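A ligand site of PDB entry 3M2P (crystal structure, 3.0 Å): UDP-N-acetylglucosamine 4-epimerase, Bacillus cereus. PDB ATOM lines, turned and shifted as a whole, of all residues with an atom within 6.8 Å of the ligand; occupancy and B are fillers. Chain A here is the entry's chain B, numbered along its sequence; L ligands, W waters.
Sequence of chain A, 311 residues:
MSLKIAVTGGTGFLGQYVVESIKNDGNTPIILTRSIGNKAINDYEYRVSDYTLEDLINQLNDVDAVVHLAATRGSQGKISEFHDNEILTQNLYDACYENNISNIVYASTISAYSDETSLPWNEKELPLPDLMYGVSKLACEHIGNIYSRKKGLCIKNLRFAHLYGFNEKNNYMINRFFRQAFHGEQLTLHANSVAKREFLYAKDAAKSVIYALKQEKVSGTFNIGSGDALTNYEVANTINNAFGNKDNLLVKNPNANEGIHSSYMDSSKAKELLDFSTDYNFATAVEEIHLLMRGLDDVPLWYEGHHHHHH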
ATOM      1  N   THR A   8      -5.319 -10.077  -1.502  1.00  0.00           N
ATOM      2  CA  THR A   8      -5.063 -11.471  -1.794  1.00  0.00           C
ATOM      3  C   THR A   8      -3.853 -11.874  -0.967  1.00  0.00           C
ATOM      4  O   THR A   8      -2.948 -11.069  -0.773  1.00  0.00           O
ATOM      5  CB  THR A   8      -4.771 -11.701  -3.296  1.00  0.00           C
ATOM      6  OG1 THR A   8      -3.461 -11.222  -3.603  1.00  0.00           O
ATOM      7  CG2 THR A   8      -5.783 -10.967  -4.168  1.00  0.00           C
ATOM      8  N   GLY A   9      -3.849 -13.110  -0.469  1.00  0.00           N
ATOM      9  CA  GLY A   9      -2.806 -13.547   0.429  1.00  0.00           C
ATOM     10  C   GLY A   9      -2.789 -12.705   1.696  1.00  0.00           C
ATOM     11  O   GLY A   9      -1.752 -12.590   2.358  1.00  0.00           O
ATOM     12  N   GLY A  10      -3.943 -12.109   2.018  1.00  0.00           N
ATOM     13  CA  GLY A  10      -4.097 -11.246   3.169  1.00  0.00           C
ATOM     14  C   GLY A  10      -3.879 -12.059   4.416  1.00  0.00           C
ATOM     15  O   GLY A  10      -3.789 -11.536   5.536  1.00  0.00           O
ATOM     16  N   THR A  11      -3.789 -13.359   4.206  1.00  0.00           N
ATOM     17  CA  THR A  11      -3.590 -14.353   5.244  1.00  0.00           C
ATOM     18  C   THR A  11      -2.123 -14.517   5.655  1.00  0.00           C
ATOM     19  O   THR A  11      -1.811 -14.628   6.833  1.00  0.00           O
ATOM     20  CB  THR A  11      -4.132 -15.704   4.753  1.00  0.00           C
ATOM     21  OG1 THR A  11      -5.549 -15.746   4.963  1.00  0.00           O
ATOM     22  CG2 THR A  11      -3.425 -16.867   5.464  1.00  0.00           C
ATOM     23  N   GLY A  12      -1.215 -14.551   4.680  1.00  0.00           N
ATOM     24  CA  GLY A  12       0.160 -14.917   4.933  1.00  0.00           C
ATOM     25  C   GLY A  12       0.995 -13.916   5.696  1.00  0.00           C
ATOM     26  O   GLY A  12       0.471 -12.929   6.224  1.00  0.00           O
ATOM     27  N   PHE A  13       2.306 -14.158   5.740  1.00  0.00           N
ATOM     28  CA  PHE A  13       3.240 -13.286   6.439  1.00  0.00           C
ATOM     29  C   PHE A  13       2.987 -11.794   6.135  1.00  0.00           C
ATOM     30  O   PHE A  13       2.280 -11.130   6.896  1.00  0.00           O
ATOM     31  CB  PHE A  13       4.683 -13.680   6.123  1.00  0.00           C
ATOM     32  CG  PHE A  13       5.710 -12.957   6.941  1.00  0.00           C
ATOM     33  CD1 PHE A  13       5.583 -12.866   8.320  1.00  0.00           C
ATOM     34  CD2 PHE A  13       6.824 -12.385   6.337  1.00  0.00           C
ATOM     35  CE1 PHE A  13       6.528 -12.204   9.068  1.00  0.00           C
ATOM     36  CE2 PHE A  13       7.776 -11.720   7.078  1.00  0.00           C
ATOM     37  CZ  PHE A  13       7.626 -11.628   8.450  1.00  0.00           C
ATOM     38  N   LEU A  14       3.541 -11.297   5.034  1.00  0.00           N
ATOM     39  CA  LEU A  14       3.369  -9.903   4.591  1.00  0.00           C
ATOM     40  C   LEU A  14       1.910  -9.444   4.653  1.00  0.00           C
ATOM     41  O   LEU A  14       1.633  -8.299   4.970  1.00  0.00           O
ATOM     42  CB  LEU A  14       3.872  -9.728   3.157  1.00  0.00           C
ATOM     43  CG  LEU A  14       4.456  -8.381   2.701  1.00  0.00           C
ATOM     44  CD1 LEU A  14       4.082  -8.104   1.248  1.00  0.00           C
ATOM     45  CD2 LEU A  14       4.010  -7.244   3.590  1.00  0.00           C
ATOM     46  N   GLY A  15       0.991 -10.341   4.319  1.00  0.00           N
ATOM     47  CA  GLY A  15      -0.429 -10.053   4.389  1.00  0.00           C
ATOM     48  C   GLY A  15      -0.888  -9.466   5.705  1.00  0.00           C
ATOM     49  O   GLY A  15      -1.464  -8.381   5.736  1.00  0.00           O
ATOM     50  N   LEU A  32      -8.803 -11.787   0.901  1.00  0.00           N
ATOM     51  CA  LEU A  32      -9.240 -12.890   0.057  1.00  0.00           C
ATOM     52  C   LEU A  32      -8.357 -14.078   0.386  1.00  0.00           C
ATOM     53  O   LEU A  32      -7.173 -13.908   0.634  1.00  0.00           O
ATOM     54  CB  LEU A  32      -9.141 -12.537  -1.427  1.00  0.00           C
ATOM     55  CG  LEU A  32     -10.349 -11.894  -2.105  1.00  0.00           C
ATOM     56  CD1 LEU A  32     -10.780 -10.625  -1.403  1.00  0.00           C
ATOM     57  CD2 LEU A  32     -10.048 -11.598  -3.554  1.00  0.00           C
ATOM     58  N   THR A  33      -8.938 -15.277   0.393  1.00  0.00           N
ATOM     59  CA  THR A  33      -8.196 -16.475   0.786  1.00  0.00           C
ATOM     60  C   THR A  33      -8.850 -17.725   0.191  1.00  0.00           C
ATOM     61  O   THR A  33     -10.002 -17.685  -0.213  1.00  0.00           O
ATOM     62  CB  THR A  33      -8.109 -16.587   2.316  1.00  0.00           C
ATOM     63  OG1 THR A  33      -7.658 -17.892   2.692  1.00  0.00           O
ATOM     64  CG2 THR A  33      -9.463 -16.298   2.952  1.00  0.00           C
ATOM     65  N   ARG A  34      -8.109 -18.810   0.114  1.00  0.00           N
ATOM     66  CA  ARG A  34      -8.634 -20.038  -0.476  1.00  0.00           C
ATOM     67  C   ARG A  34      -9.486 -20.822   0.534  1.00  0.00           C
ATOM     68  O   ARG A  34     -10.275 -21.689   0.164  1.00  0.00           O
ATOM     69  CB  ARG A  34      -7.493 -20.920  -0.998  1.00  0.00           C
ATOM     70  CG  ARG A  34      -6.626 -20.252  -2.054  1.00  0.00           C
ATOM     71  CD  ARG A  34      -5.734 -21.243  -2.794  1.00  0.00           C
ATOM     72  NE  ARG A  34      -4.458 -21.603  -2.151  1.00  0.00           N
ATOM     73  CZ  ARG A  34      -3.976 -21.129  -0.999  1.00  0.00           C
ATOM     74  NH1 ARG A  34      -2.797 -21.577  -0.562  1.00  0.00           N
ATOM     75  NH2 ARG A  34      -4.630 -20.234  -0.271  1.00  0.00           N
ATOM     76  N   SER A  35      -9.310 -20.497   1.814  1.00  0.00           N
ATOM     77  CA  SER A  35      -9.965 -21.250   2.871  1.00  0.00           C
ATOM     78  C   SER A  35      -9.870 -20.471   4.181  1.00  0.00           C
ATOM     79  O   SER A  35      -9.023 -19.592   4.312  1.00  0.00           O
ATOM     80  CB  SER A  35      -9.292 -22.624   3.023  1.00  0.00           C
ATOM     81  OG  SER A  35      -9.836 -23.386   4.095  1.00  0.00           O
ATOM     82  N   TYR A  51     -10.481 -18.064  -6.715  1.00  0.00           N
ATOM     83  CA  TYR A  51      -9.777 -17.221  -7.674  1.00  0.00           C
ATOM     84  C   TYR A  51     -10.069 -17.572  -9.115  1.00  0.00           C
ATOM     85  O   TYR A  51      -9.196 -17.428  -9.967  1.00  0.00           O
ATOM     86  CB  TYR A  51      -8.270 -17.237  -7.446  1.00  0.00           C
ATOM     87  CG  TYR A  51      -7.843 -16.632  -6.126  1.00  0.00           C
ATOM     88  CD1 TYR A  51      -7.470 -15.296  -6.039  1.00  0.00           C
ATOM     89  CD2 TYR A  51      -7.786 -17.406  -4.988  1.00  0.00           C
ATOM     90  CE1 TYR A  51      -7.076 -14.757  -4.834  1.00  0.00           C
ATOM     91  CE2 TYR A  51      -7.385 -16.873  -3.779  1.00  0.00           C
ATOM     92  CZ  TYR A  51      -7.040 -15.550  -3.713  1.00  0.00           C
ATOM     93  OH  TYR A  51      -6.650 -15.045  -2.499  1.00  0.00           O
ATOM     94  N   LEU A  69      -1.051  -9.925  -3.134  1.00  0.00           N
ATOM     95  CA  LEU A  69       0.042 -10.638  -2.457  1.00  0.00           C
ATOM     96  C   LEU A  69      -0.005 -12.164  -2.624  1.00  0.00           C
ATOM     97  O   LEU A  69       0.988 -12.847  -2.381  1.00  0.00           O
ATOM     98  CB  LEU A  69       0.081 -10.278  -0.977  1.00  0.00           C
ATOM     99  CG  LEU A  69       0.184  -8.787  -0.682  1.00  0.00           C
ATOM    100  CD1 LEU A  69      -0.115  -8.506   0.781  1.00  0.00           C
ATOM    101  CD2 LEU A  69       1.548  -8.244  -1.066  1.00  0.00           C
ATOM    102  N   ALA A  70      -1.152 -12.698  -3.050  1.00  0.00           N
ATOM    103  CA  ALA A  70      -1.331 -14.134  -3.254  1.00  0.00           C
ATOM    104  C   ALA A  70      -0.294 -14.698  -4.207  1.00  0.00           C
ATOM    105  O   ALA A  70      -0.246 -14.325  -5.367  1.00  0.00           O
ATOM    106  CB  ALA A  70      -2.693 -14.427  -3.794  1.00  0.00           C
ATOM    107  N   ALA A  71       0.530 -15.613  -3.698  1.00  0.00           N
ATOM    108  CA  ALA A  71       1.628 -16.179  -4.484  1.00  0.00           C
ATOM    109  C   ALA A  71       2.064 -17.553  -3.978  1.00  0.00           C
ATOM    110  O   ALA A  71       1.709 -17.957  -2.870  1.00  0.00           O
ATOM    111  CB  ALA A  71       2.804 -15.216  -4.494  1.00  0.00           C
ATOM    112  N   THR A  72       2.843 -18.250  -4.791  1.00  0.00           N
ATOM    113  CA  THR A  72       3.318 -19.585  -4.452  1.00  0.00           C
ATOM    114  C   THR A  72       4.841 -19.636  -4.456  1.00  0.00           C
ATOM    115  O   THR A  72       5.484 -19.017  -5.309  1.00  0.00           O
ATOM    116  CB  THR A  72       2.757 -20.651  -5.400  1.00  0.00           C
ATOM    117  OG1 THR A  72       1.478 -21.071  -4.908  1.00  0.00           O
ATOM    118  CG2 THR A  72       3.673 -21.845  -5.468  1.00  0.00           C
ATOM    119  N   ARG A  73       5.399 -20.360  -3.487  1.00  0.00           N
ATOM    120  CA  ARG A  73       6.842 -20.405  -3.263  1.00  0.00           C
ATOM    121  C   ARG A  73       7.551 -21.314  -4.262  1.00  0.00           C
ATOM    122  O   ARG A  73       8.621 -20.970  -4.793  1.00  0.00           O
ATOM    123  CB  ARG A  73       7.176 -20.889  -1.841  1.00  0.00           C
ATOM    124  CG  ARG A  73       6.807 -19.939  -0.706  1.00  0.00           C
ATOM    125  CD  ARG A  73       7.595 -20.279   0.567  1.00  0.00           C
ATOM    126  NE  ARG A  73       7.829 -21.720   0.728  1.00  0.00           N
ATOM    127  CZ  ARG A  73       8.988 -22.337   0.491  1.00  0.00           C
ATOM    128  NH1 ARG A  73      10.048 -21.643   0.066  1.00  0.00           N
ATOM    129  NH2 ARG A  73       9.102 -23.651   0.676  1.00  0.00           N
ATOM    130  N   ASP A  84       0.129 -21.250 -11.931  1.00  0.00           N
ATOM    131  CA  ASP A  84      -1.106 -20.932 -11.264  1.00  0.00           C
ATOM    132  C   ASP A  84      -1.128 -19.472 -10.839  1.00  0.00           C
ATOM    133  O   ASP A  84      -2.093 -18.775 -11.062  1.00  0.00           O
ATOM    134  CB  ASP A  84      -1.283 -21.840 -10.056  1.00  0.00           C
ATOM    135  CG  ASP A  84      -2.703 -22.266  -9.877  1.00  0.00           C
ATOM    136  OD1 ASP A  84      -3.186 -23.020 -10.757  1.00  0.00           O
ATOM    137  OD2 ASP A  84      -3.331 -21.830  -8.887  1.00  0.00           O
ATOM    138  N   ASN A  85      -0.044 -19.029 -10.208  1.00  0.00           N
ATOM    139  CA  ASN A  85       0.071 -17.638  -9.804  1.00  0.00           C
ATOM    140  C   ASN A  85      -0.214 -16.703 -10.976  1.00  0.00           C
ATOM    141  O   ASN A  85      -0.730 -15.601 -10.800  1.00  0.00           O
ATOM    142  CB  ASN A  85       1.475 -17.380  -9.287  1.00  0.00           C
ATOM    143  CG  ASN A  85       1.717 -18.028  -7.940  1.00  0.00           C
ATOM    144  OD1 ASN A  85       2.803 -18.539  -7.661  1.00  0.00           O
ATOM    145  ND2 ASN A  85       0.681 -18.009  -7.086  1.00  0.00           N
ATOM    146  N   LEU A  88      -4.013 -16.875 -11.996  1.00  0.00           N
ATOM    147  CA  LEU A  88      -4.648 -16.156 -10.903  1.00  0.00           C
ATOM    148  C   LEU A  88      -4.478 -14.654 -11.067  1.00  0.00           C
ATOM    149  O   LEU A  88      -5.421 -13.896 -10.885  1.00  0.00           O
ATOM    150  CB  LEU A  88      -4.028 -16.612  -9.574  1.00  0.00           C
ATOM    151  CG  LEU A  88      -4.524 -16.022  -8.263  1.00  0.00           C
ATOM    152  CD1 LEU A  88      -3.986 -16.864  -7.104  1.00  0.00           C
ATOM    153  CD2 LEU A  88      -4.115 -14.567  -8.089  1.00  0.00           C
ATOM    154  N   ALA A 107       3.050  -7.549  -5.388  1.00  0.00           N
ATOM    155  CA  ALA A 107       4.250  -7.972  -4.675  1.00  0.00           C
ATOM    156  C   ALA A 107       5.200  -8.721  -5.618  1.00  0.00           C
ATOM    157  O   ALA A 107       5.067  -9.911  -5.870  1.00  0.00           O
ATOM    158  CB  ALA A 107       3.885  -8.845  -3.483  1.00  0.00           C
ATOM    159  N   LEU A 163      12.455 -10.181   3.154  1.00  0.00           N
ATOM    160  CA  LEU A 163      11.650  -9.779   4.312  1.00  0.00           C
ATOM    161  C   LEU A 163      11.846 -10.619   5.583  1.00  0.00           C
ATOM    162  O   LEU A 163      11.792 -11.853   5.553  1.00  0.00           O
ATOM    163  CB  LEU A 163      10.175  -9.746   3.974  1.00  0.00           C
ATOM    164  CG  LEU A 163       9.771  -9.341   2.560  1.00  0.00           C
ATOM    165  CD1 LEU A 163      10.122 -10.467   1.554  1.00  0.00           C
ATOM    166  CD2 LEU A 163       8.276  -9.029   2.521  1.00  0.00           C
ATOM    167  N   GLU A 168       7.605 -16.368  12.079  1.00  0.00           N
ATOM    168  CA  GLU A 168       7.789 -16.855  10.722  1.00  0.00           C
ATOM    169  C   GLU A 168       7.875 -18.390  10.578  1.00  0.00           C
ATOM    170  O   GLU A 168       6.971 -19.122  10.971  1.00  0.00           O
ATOM    171  CB  GLU A 168       9.065 -16.232  10.156  1.00  0.00           C
ATOM    172  CG  GLU A 168       8.872 -14.974   9.345  1.00  0.00           C
ATOM    173  CD  GLU A 168       9.205 -15.181   7.880  1.00  0.00           C
ATOM    174  OE1 GLU A 168      10.351 -14.890   7.489  1.00  0.00           O
ATOM    175  OE2 GLU A 168       8.333 -15.655   7.126  1.00  0.00           O
HETATM  176  N1  LIG L   1      -2.542 -18.028  -1.632  1.00  0.00           N
HETATM  177  C1  LIG L   1      -1.406 -18.658  -2.127  1.00  0.00           C
HETATM  178  N2  LIG L   1      -1.437 -19.335  -3.453  1.00  0.00           N
HETATM  179  C2  LIG L   1      -2.662 -19.322  -4.220  1.00  0.00           C
HETATM  180  C3  LIG L   1      -3.808 -18.666  -3.721  1.00  0.00           C
HETATM  181  C4  LIG L   1      -3.787 -18.010  -2.431  1.00  0.00           C
HETATM  182  O1  LIG L   1      -0.405 -18.689  -1.488  1.00  0.00           O
HETATM  183  O2  LIG L   1      -2.719 -19.957  -5.489  1.00  0.00           O
HETATM  184  C5  LIG L   1      -2.487 -17.318  -0.323  1.00  0.00           C
HETATM  185  C6  LIG L   1      -2.721 -18.179   0.930  1.00  0.00           C
HETATM  186  O3  LIG L   1      -3.973 -18.166   1.609  1.00  0.00           O
HETATM  187  C7  LIG L   1      -1.356 -17.930   1.707  1.00  0.00           C
HETATM  188  C8  LIG L   1      -0.937 -16.503   1.160  1.00  0.00           C
HETATM  189  O4  LIG L   1      -1.264 -16.640  -0.230  1.00  0.00           O
HETATM  190  O5  LIG L   1      -1.249 -18.189   3.084  1.00  0.00           O
HETATM  191  C9  LIG L   1       0.389 -15.759   1.545  1.00  0.00           C
HETATM  192  O6  LIG L   1       1.648 -16.413   1.328  1.00  0.00           O
HETATM  193  P1  LIG L   1       2.960 -16.052   2.340  1.00  0.00           P
HETATM  194  O7  LIG L   1       2.706 -16.606   3.908  1.00  0.00           O
HETATM  195  O8  LIG L   1       4.148 -16.717   1.803  1.00  0.00           O
HETATM  196  O9  LIG L   1       3.128 -14.381   2.328  1.00  0.00           O
HETATM  197  P2  LIG L   1       4.570 -13.580   1.980  1.00  0.00           P
HETATM  198  O10 LIG L   1       4.374 -12.686   0.587  1.00  0.00           O
HETATM  199  O11 LIG L   1       4.948 -12.577   3.241  1.00  0.00           O
HETATM  200  O12 LIG L   1       5.662 -14.545   1.805  1.00  0.00           O
HETATM  201  O   HOH W   1       4.747 -11.895  -1.733  1.00  0.00           O
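An oxygen (O11) of the ligand sits at hydrogen-bond distance from the backbone NH (N) of Leu 14.
A nitrogen (N2) of the ligand sits close to the backbone carbonyl oxygen (O) of Ala 71 (3.5 Å).
An oxygen (O3) of the ligand is in hydrogen-bond range of the guanidinium group (NH2) of Arg 34, at 2.9 Å.
O7 of the ligand sits at hydrogen-bond distance from N of Phe 13 (3.1 Å).
The backbone NH (N) of Thr 72 sits at hydrogen-bond distance from the side-chain amide oxygen (OD1) of Asn 85, 2.9 Å away.
OG1 of Thr 33 lies within hydrogen-bond range of O of Ser 35.
OG1 of Thr 8 sits at hydrogen-bond distance from N of Ala 70 (2.8 Å).
Residues that only touch the ligand: Gly 9, Thr 11, Gly 12, Thr 33, Ala 70, Thr 72, Asp 84 and Leu 88.
Hydrophobic or aromatic side chains within 4 Å of the ligand: Phe 13, Leu 14, Ala 70 and Leu 88.
Of the 24 residues printed, 12 come within 4 Å of the ligand.
The nearest printed residue that does not touch the ligand is Tyr 51 (4.002 Å).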
